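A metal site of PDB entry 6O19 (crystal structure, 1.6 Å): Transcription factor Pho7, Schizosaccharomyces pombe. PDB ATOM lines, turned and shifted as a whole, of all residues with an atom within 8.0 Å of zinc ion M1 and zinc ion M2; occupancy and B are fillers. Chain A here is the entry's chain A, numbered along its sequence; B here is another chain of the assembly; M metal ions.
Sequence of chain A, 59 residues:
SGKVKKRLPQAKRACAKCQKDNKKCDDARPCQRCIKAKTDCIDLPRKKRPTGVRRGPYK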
ATOM      1  N   ALA A  11      13.522 -16.487   6.013  1.00  0.00           N
ATOM      2  CA  ALA A  11      14.264 -17.571   5.387  1.00  0.00           C
ATOM      3  C   ALA A  11      14.192 -17.431   3.869  1.00  0.00           C
ATOM      4  O   ALA A  11      13.201 -16.938   3.317  1.00  0.00           O
ATOM      5  CB  ALA A  11      13.701 -18.915   5.818  1.00  0.00           C
ATOM      6  N   ARG A  13      13.699 -19.779   1.808  1.00  0.00           N
ATOM      7  CA  ARG A  13      12.465 -20.498   1.559  1.00  0.00           C
ATOM      8  C   ARG A  13      12.142 -21.345   2.789  1.00  0.00           C
ATOM      9  O   ARG A  13      13.025 -21.707   3.562  1.00  0.00           O
ATOM     10  CB  ARG A  13      12.544 -21.375   0.289  1.00  0.00           C
ATOM     11  CG  ARG A  13      13.224 -22.705   0.509  1.00  0.00           C
ATOM     12  CD  ARG A  13      13.528 -23.452  -0.799  1.00  0.00           C
ATOM     13  NE  ARG A  13      12.476 -23.370  -1.820  1.00  0.00           N
ATOM     14  CZ  ARG A  13      11.342 -24.087  -1.797  1.00  0.00           C
ATOM     15  NH1 ARG A  13      11.072 -24.902  -0.786  1.00  0.00           N
ATOM     16  NH2 ARG A  13      10.474 -23.964  -2.790  1.00  0.00           N
ATOM     17  N   ALA A  14      10.861 -21.636   2.958  1.00  0.00           N
ATOM     18  CA  ALA A  14      10.406 -22.423   4.099  1.00  0.00           C
ATOM     19  C   ALA A  14      10.202 -23.875   3.692  1.00  0.00           C
ATOM     20  O   ALA A  14       9.719 -24.166   2.599  1.00  0.00           O
ATOM     21  CB  ALA A  14       9.112 -21.845   4.673  1.00  0.00           C
ATOM     22  N   CYS A  15      10.599 -24.780   4.574  1.00  0.00           N
ATOM     23  CA  CYS A  15      10.387 -26.201   4.363  1.00  0.00           C
ATOM     24  C   CYS A  15       8.906 -26.549   4.565  1.00  0.00           C
ATOM     25  O   CYS A  15       8.117 -25.768   5.098  1.00  0.00           O
ATOM     26  CB  CYS A  15      11.249 -27.016   5.330  1.00  0.00           C
ATOM     27  SG  CYS A  15      10.643 -26.955   7.076  1.00  0.00           S
ATOM     28  N   ALA A  16       8.562 -27.780   4.188  1.00  0.00           N
ATOM     29  CA  ALA A  16       7.161 -28.163   4.161  1.00  0.00           C
ATOM     30  C   ALA A  16       6.519 -28.089   5.547  1.00  0.00           C
ATOM     31  O   ALA A  16       5.358 -27.686   5.662  1.00  0.00           O
ATOM     32  CB  ALA A  16       7.004 -29.561   3.558  1.00  0.00           C
ATOM     33  N   LYS A  17       7.242 -28.475   6.600  1.00  0.00           N
ATOM     34  CA  LYS A  17       6.632 -28.447   7.925  1.00  0.00           C
ATOM     35  C   LYS A  17       6.439 -27.020   8.426  1.00  0.00           C
ATOM     36  O   LYS A  17       5.383 -26.688   8.977  1.00  0.00           O
ATOM     37  CB  LYS A  17       7.429 -29.259   8.932  1.00  0.00           C
ATOM     38  CG  LYS A  17       6.828 -29.179  10.325  1.00  0.00           C
ATOM     39  CD  LYS A  17       7.602 -30.009  11.308  1.00  0.00           C
ATOM     40  CE  LYS A  17       7.412 -29.511  12.732  1.00  0.00           C
ATOM     41  NZ  LYS A  17       5.984 -29.609  13.165  1.00  0.00           N
ATOM     42  N   CYS A  18       7.434 -26.143   8.224  1.00  0.00           N
ATOM     43  CA  CYS A  18       7.251 -24.744   8.607  1.00  0.00           C
ATOM     44  C   CYS A  18       6.135 -24.100   7.797  1.00  0.00           C
ATOM     45  O   CYS A  18       5.396 -23.249   8.318  1.00  0.00           O
ATOM     46  CB  CYS A  18       8.561 -23.976   8.439  1.00  0.00           C
ATOM     47  SG  CYS A  18       9.789 -24.394   9.716  1.00  0.00           S
ATOM     48  N   GLN A  19       5.985 -24.482   6.531  1.00  0.00           N
ATOM     49  CA  GLN A  19       4.855 -24.001   5.736  1.00  0.00           C
ATOM     50  C   GLN A  19       3.527 -24.460   6.338  1.00  0.00           C
ATOM     51  O   GLN A  19       2.606 -23.656   6.514  1.00  0.00           O
ATOM     52  CB  GLN A  19       4.980 -24.472   4.293  1.00  0.00           C
ATOM     53  CG  GLN A  19       6.093 -23.780   3.511  1.00  0.00           C
ATOM     54  CD  GLN A  19       6.364 -24.425   2.173  1.00  0.00           C
ATOM     55  OE1 GLN A  19       6.321 -25.652   2.037  1.00  0.00           O
ATOM     56  NE2 GLN A  19       6.644 -23.603   1.182  1.00  0.00           N
ATOM     57  N   LYS A  23       5.087 -21.282  10.623  1.00  0.00           N
ATOM     58  CA  LYS A  23       6.098 -20.894  11.596  1.00  0.00           C
ATOM     59  C   LYS A  23       7.414 -20.529  10.892  1.00  0.00           C
ATOM     60  O   LYS A  23       7.562 -20.691   9.680  1.00  0.00           O
ATOM     61  CB  LYS A  23       6.298 -22.011  12.630  1.00  0.00           C
ATOM     62  CG  LYS A  23       5.124 -22.202  13.582  1.00  0.00           C
ATOM     63  CD  LYS A  23       4.901 -20.962  14.434  1.00  0.00           C
ATOM     64  CE  LYS A  23       3.944 -21.227  15.585  1.00  0.00           C
ATOM     65  NZ  LYS A  23       3.602 -19.941  16.282  1.00  0.00           N
ATOM     66  N   LYS A  24       8.369 -20.049  11.682  1.00  0.00           N
ATOM     67  CA  LYS A  24       9.602 -19.450  11.174  1.00  0.00           C
ATOM     68  C   LYS A  24      10.589 -20.533  10.768  1.00  0.00           C
ATOM     69  O   LYS A  24      11.074 -21.277  11.625  1.00  0.00           O
ATOM     70  CB  LYS A  24      10.189 -18.538  12.251  1.00  0.00           C
ATOM     71  CG  LYS A  24      11.509 -17.870  11.896  1.00  0.00           C
ATOM     72  CD  LYS A  24      11.263 -16.646  11.040  1.00  0.00           C
ATOM     73  CE  LYS A  24      12.568 -16.009  10.586  1.00  0.00           C
ATOM     74  NZ  LYS A  24      13.172 -16.818   9.491  1.00  0.00           N
ATOM     75  N   CYS A  25      10.909 -20.608   9.486  1.00  0.00           N
ATOM     76  CA  CYS A  25      11.944 -21.528   8.997  1.00  0.00           C
ATOM     77  C   CYS A  25      13.308 -20.826   9.084  1.00  0.00           C
ATOM     78  O   CYS A  25      13.442 -19.752   9.689  1.00  0.00           O
ATOM     79  CB  CYS A  25      11.609 -22.013   7.585  1.00  0.00           C
ATOM     80  SG  CYS A  25      12.499 -23.520   7.062  1.00  0.00           S
ATOM     81  N   ASP A  26      14.343 -21.431   8.518  1.00  0.00           N
ATOM     82  CA  ASP A  26      15.652 -20.797   8.440  1.00  0.00           C
ATOM     83  C   ASP A  26      16.376 -21.357   7.223  1.00  0.00           C
ATOM     84  O   ASP A  26      15.764 -22.025   6.375  1.00  0.00           O
ATOM     85  CB  ASP A  26      16.435 -20.955   9.756  1.00  0.00           C
ATOM     86  CG  ASP A  26      16.586 -22.415  10.182  1.00  0.00           C
ATOM     87  OD1 ASP A  26      17.305 -23.154   9.505  1.00  0.00           O
ATOM     88  OD2 ASP A  26      15.988 -22.805  11.211  1.00  0.00           O
ATOM     89  N   ASP A  27      17.671 -21.058   7.097  1.00  0.00           N
ATOM     90  CA  ASP A  27      18.397 -21.461   5.899  1.00  0.00           C
ATOM     91  C   ASP A  27      19.235 -22.720   6.111  1.00  0.00           C
ATOM     92  O   ASP A  27      19.928 -23.143   5.170  1.00  0.00           O
ATOM     93  CB  ASP A  27      19.266 -20.304   5.415  1.00  0.00           C
ATOM     94  CG  ASP A  27      18.438 -19.068   5.072  1.00  0.00           C
ATOM     95  OD1 ASP A  27      17.328 -19.240   4.500  1.00  0.00           O
ATOM     96  OD2 ASP A  27      18.859 -17.935   5.377  1.00  0.00           O
ATOM     97  N   ALA A  28      19.167 -23.328   7.290  1.00  0.00           N
ATOM     98  CA  ALA A  28      19.767 -24.638   7.501  1.00  0.00           C
ATOM     99  C   ALA A  28      18.842 -25.720   6.950  1.00  0.00           C
ATOM    100  O   ALA A  28      17.618 -25.579   6.942  1.00  0.00           O
ATOM    101  CB  ALA A  28      19.990 -24.887   8.990  1.00  0.00           C
ATOM    102  N   ARG A  29      19.448 -26.828   6.508  1.00  0.00           N
ATOM    103  CA  ARG A  29      18.672 -28.001   6.103  1.00  0.00           C
ATOM    104  C   ARG A  29      19.334 -29.251   6.669  1.00  0.00           C
ATOM    105  O   ARG A  29      20.427 -29.621   6.238  1.00  0.00           O
ATOM    106  CB  ARG A  29      18.542 -28.092   4.583  1.00  0.00           C
ATOM    107  CG  ARG A  29      17.612 -27.041   3.983  1.00  0.00           C
ATOM    108  CD  ARG A  29      16.195 -27.248   4.450  1.00  0.00           C
ATOM    109  NE  ARG A  29      15.237 -26.359   3.773  1.00  0.00           N
ATOM    110  CZ  ARG A  29      14.847 -25.169   4.240  1.00  0.00           C
ATOM    111  NH1 ARG A  29      15.329 -24.706   5.397  1.00  0.00           N
ATOM    112  NH2 ARG A  29      13.967 -24.447   3.555  1.00  0.00           N
ATOM    113  N   PRO A  30      18.702 -29.936   7.650  1.00  0.00           N
ATOM    114  CA  PRO A  30      17.368 -29.626   8.185  1.00  0.00           C
ATOM    115  C   PRO A  30      17.292 -28.313   8.959  1.00  0.00           C
ATOM    116  O   PRO A  30      18.290 -27.902   9.556  1.00  0.00           O
ATOM    117  CB  PRO A  30      17.097 -30.817   9.117  1.00  0.00           C
ATOM    118  CG  PRO A  30      18.496 -31.306   9.522  1.00  0.00           C
ATOM    119  CD  PRO A  30      19.307 -31.123   8.275  1.00  0.00           C
ATOM    120  N   CYS A  31      16.125 -27.670   8.935  1.00  0.00           N
ATOM    121  CA  CYS A  31      15.958 -26.410   9.654  1.00  0.00           C
ATOM    122  C   CYS A  31      15.862 -26.667  11.153  1.00  0.00           C
ATOM    123  O   CYS A  31      15.655 -27.797  11.601  1.00  0.00           O
ATOM    124  CB  CYS A  31      14.715 -25.679   9.136  1.00  0.00           C
ATOM    125  SG  CYS A  31      13.135 -26.379   9.681  1.00  0.00           S
ATOM    126  N   GLN A  32      16.011 -25.605  11.938  1.00  0.00           N
ATOM    127  CA  GLN A  32      16.087 -25.795  13.390  1.00  0.00           C
ATOM    128  C   GLN A  32      14.774 -26.353  13.945  1.00  0.00           C
ATOM    129  O   GLN A  32      14.786 -27.188  14.853  1.00  0.00           O
ATOM    130  CB  GLN A  32      16.461 -24.494  14.083  1.00  0.00           C
ATOM    131  CG  GLN A  32      17.843 -23.977  13.672  1.00  0.00           C
ATOM    132  CD  GLN A  32      18.891 -25.073  13.696  1.00  0.00           C
ATOM    133  OE1 GLN A  32      19.207 -25.607  14.761  1.00  0.00           O
ATOM    134  NE2 GLN A  32      19.429 -25.421  12.532  1.00  0.00           N
ATOM    135  N   ARG A  33      13.634 -25.927  13.395  1.00  0.00           N
ATOM    136  CA  ARG A  33      12.360 -26.420  13.919  1.00  0.00           C
ATOM    137  C   ARG A  33      12.196 -27.909  13.655  1.00  0.00           C
ATOM    138  O   ARG A  33      11.611 -28.630  14.472  1.00  0.00           O
ATOM    139  CB  ARG A  33      11.178 -25.639  13.336  1.00  0.00           C
ATOM    140  CG  ARG A  33      10.938 -24.268  13.955  1.00  0.00           C
ATOM    141  CD  ARG A  33       9.582 -23.673  13.499  1.00  0.00           C
ATOM    142  NE  ARG A  33       8.434 -24.269  14.186  1.00  0.00           N
ATOM    143  CZ  ARG A  33       7.534 -25.067  13.623  1.00  0.00           C
ATOM    144  NH1 ARG A  33       7.632 -25.382  12.327  1.00  0.00           N
ATOM    145  NH2 ARG A  33       6.532 -25.552  14.333  1.00  0.00           N
ATOM    146  N   CYS A  34      12.688 -28.390  12.500  1.00  0.00           N
ATOM    147  CA  CYS A  34      12.572 -29.805  12.186  1.00  0.00           C
ATOM    148  C   CYS A  34      13.528 -30.645  13.045  1.00  0.00           C
ATOM    149  O   CYS A  34      13.176 -31.766  13.444  1.00  0.00           O
ATOM    150  CB  CYS A  34      12.836 -30.040  10.694  1.00  0.00           C
ATOM    151  SG  CYS A  34      11.372 -29.626   9.660  1.00  0.00           S
ATOM    152  N   ILE A  35      14.718 -30.118  13.341  1.00  0.00           N
ATOM    153  CA  ILE A  35      15.630 -30.849  14.233  1.00  0.00           C
ATOM    154  C   ILE A  35      14.984 -31.049  15.590  1.00  0.00           C
ATOM    155  O   ILE A  35      14.955 -32.166  16.132  1.00  0.00           O
ATOM    156  CB  ILE A  35      16.977 -30.105  14.343  1.00  0.00           C
ATOM    157  CG1 ILE A  35      17.696 -30.113  13.000  1.00  0.00           C
ATOM    158  CG2 ILE A  35      17.867 -30.772  15.397  1.00  0.00           C
ATOM    159  CD1 ILE A  35      18.928 -29.241  12.943  1.00  0.00           C
ATOM    160  N   THR A  39      11.313 -34.140  12.790  1.00  0.00           N
ATOM    161  CA  THR A  39      10.469 -34.316  11.622  1.00  0.00           C
ATOM    162  C   THR A  39      11.289 -34.110  10.347  1.00  0.00           C
ATOM    163  O   THR A  39      12.161 -33.252  10.293  1.00  0.00           O
ATOM    164  CB  THR A  39       9.310 -33.317  11.615  1.00  0.00           C
ATOM    165  OG1 THR A  39       9.834 -31.990  11.735  1.00  0.00           O
ATOM    166  CG2 THR A  39       8.348 -33.595  12.768  1.00  0.00           C
ATOM    167  N   ASP A  40      10.981 -34.918   9.327  1.00  0.00           N
ATOM    168  CA  ASP A  40      11.613 -34.773   8.023  1.00  0.00           C
ATOM    169  C   ASP A  40      11.520 -33.341   7.530  1.00  0.00           C
ATOM    170  O   ASP A  40      10.451 -32.727   7.550  1.00  0.00           O
ATOM    171  CB  ASP A  40      10.915 -35.740   7.050  1.00  0.00           C
ATOM    172  CG  ASP A  40      11.633 -35.894   5.716  1.00  0.00           C
ATOM    173  OD1 ASP A  40      12.810 -35.475   5.581  1.00  0.00           O
ATOM    174  OD2 ASP A  40      11.010 -36.443   4.785  1.00  0.00           O
ATOM    175  N   CYS A  41      12.657 -32.799   7.088  1.00  0.00           N
ATOM    176  CA  CYS A  41      12.720 -31.428   6.586  1.00  0.00           C
ATOM    177  C   CYS A  41      12.866 -31.483   5.072  1.00  0.00           C
ATOM    178  O   CYS A  41      13.948 -31.776   4.548  1.00  0.00           O
ATOM    179  CB  CYS A  41      13.886 -30.677   7.249  1.00  0.00           C
ATOM    180  SG  CYS A  41      13.953 -28.924   6.813  1.00  0.00           S
ATOM    181  N   ILE A  42      11.775 -31.201   4.360  1.00  0.00           N
ATOM    182  CA  ILE A  42      11.709 -31.358   2.904  1.00  0.00           C
ATOM    183  C   ILE A  42      11.324 -30.018   2.289  1.00  0.00           C
ATOM    184  O   ILE A  42      10.425 -29.339   2.799  1.00  0.00           O
ATOM    185  CB  ILE A  42      10.673 -32.413   2.475  1.00  0.00           C
ATOM    186  CG1 ILE A  42      10.670 -33.612   3.408  1.00  0.00           C
ATOM    187  CG2 ILE A  42      10.909 -32.847   1.028  1.00  0.00           C
ATOM    188  CD1 ILE A  42       9.343 -34.332   3.418  1.00  0.00           C
ATOM    189  N   ASP A  43      11.959 -29.671   1.168  1.00  0.00           N
ATOM    190  CA  ASP A  43      11.551 -28.508   0.377  1.00  0.00           C
ATOM    191  C   ASP A  43      10.625 -28.932  -0.764  1.00  0.00           C
ATOM    192  O   ASP A  43      10.937 -29.862  -1.516  1.00  0.00           O
ATOM    193  CB  ASP A  43      12.771 -27.776  -0.169  1.00  0.00           C
ATOM    194  CG  ASP A  43      13.427 -26.900   0.869  1.00  0.00           C
ATOM    195  OD1 ASP A  43      12.734 -26.009   1.427  1.00  0.00           O
ATOM    196  OD2 ASP A  43      14.633 -27.099   1.127  1.00  0.00           O
ATOM    197  P    DC B  12       9.898 -17.473   7.295  1.00  0.00           P
ATOM    198  OP1  DC B  12      11.231 -16.854   7.521  1.00  0.00           O
ATOM    199  OP2  DC B  12       9.702 -18.916   7.316  1.00  0.00           O
ATOM    200  O5'  DC B  12       8.853 -16.866   8.353  1.00  0.00           O
ATOM    201  C5'  DC B  12       8.782 -15.465   8.541  1.00  0.00           C
ATOM    202  C4'  DC B  12       7.636 -15.103   9.471  1.00  0.00           C
ATOM    203  O4'  DC B  12       6.371 -15.347   8.800  1.00  0.00           O
ATOM    204  C3'  DC B  12       7.565 -15.900  10.795  1.00  0.00           C
ATOM    205  O3'  DC B  12       7.083 -15.025  11.791  1.00  0.00           O
ATOM    206  C2'  DC B  12       6.516 -16.948  10.482  1.00  0.00           C
ATOM    207  C1'  DC B  12       5.544 -16.085   9.693  1.00  0.00           C
ATOM    208  N1   DC B  12       4.517 -16.798   8.899  1.00  0.00           N
ATOM    209  C2   DC B  12       3.258 -16.220   8.791  1.00  0.00           C
ATOM    210  O2   DC B  12       3.025 -15.172   9.401  1.00  0.00           O
ATOM    211  N3   DC B  12       2.302 -16.840   8.051  1.00  0.00           N
ATOM    212  C4   DC B  12       2.591 -17.965   7.392  1.00  0.00           C
ATOM    213  N4   DC B  12       1.618 -18.523   6.652  1.00  0.00           N
ATOM    214  C5   DC B  12       3.903 -18.563   7.466  1.00  0.00           C
ATOM    215  C6   DC B  12       4.828 -17.943   8.218  1.00  0.00           C
HETATM  216 ZN    ZN M   1      12.320 -28.137   8.230  1.00  0.00          ZN
HETATM  217 ZN    ZN M   2      11.555 -25.091   8.420  1.00  0.00          ZN
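NH1 of Arg 29 sits close to SG of Cys 25, at 3.5 Å. The backbone NH (N) of Cys 25 sits at hydrogen-bond distance from OP2 of DC 12 of chain B (3.0 Å). The side-chain sulfur of Cys 18 lies close to the guanidinium group of Arg 33. O of Cys 18 is in hydrogen-bond range of N of Lys 23, 3.0 Å away. The side-chain sulfur of Cys 15 lies close to the backbone NH of Lys 17, 3.8 Å away. The backbone carbonyl oxygen (O) of Cys 34 lies within hydrogen-bond range of the backbone NH (N) of Thr 39 (3.1 Å). SG of Cys 31 lies close to N of Arg 33, at 3.8 Å.
Zinc ion M2 is bound by SG of Cys 25. Zinc ion M2 is bound by SG of Cys 18 (2.3 Å). Zinc ion M2 is bound by SG of Cys 31 (2.4 Å). The side-chain sulfur (SG) of Cys 15 is bound to zinc ion M2 (2.5 Å).
Zinc ion M1 is bound by SG of Cys 34, SG of Cys 41, SG of Cys 15 and SG of Cys 31. Zinc ion M1 has four donor atoms within binding distance.
The nearest printed residue that does not touch zinc ion M2 is Asp 26 (4.6 Å).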
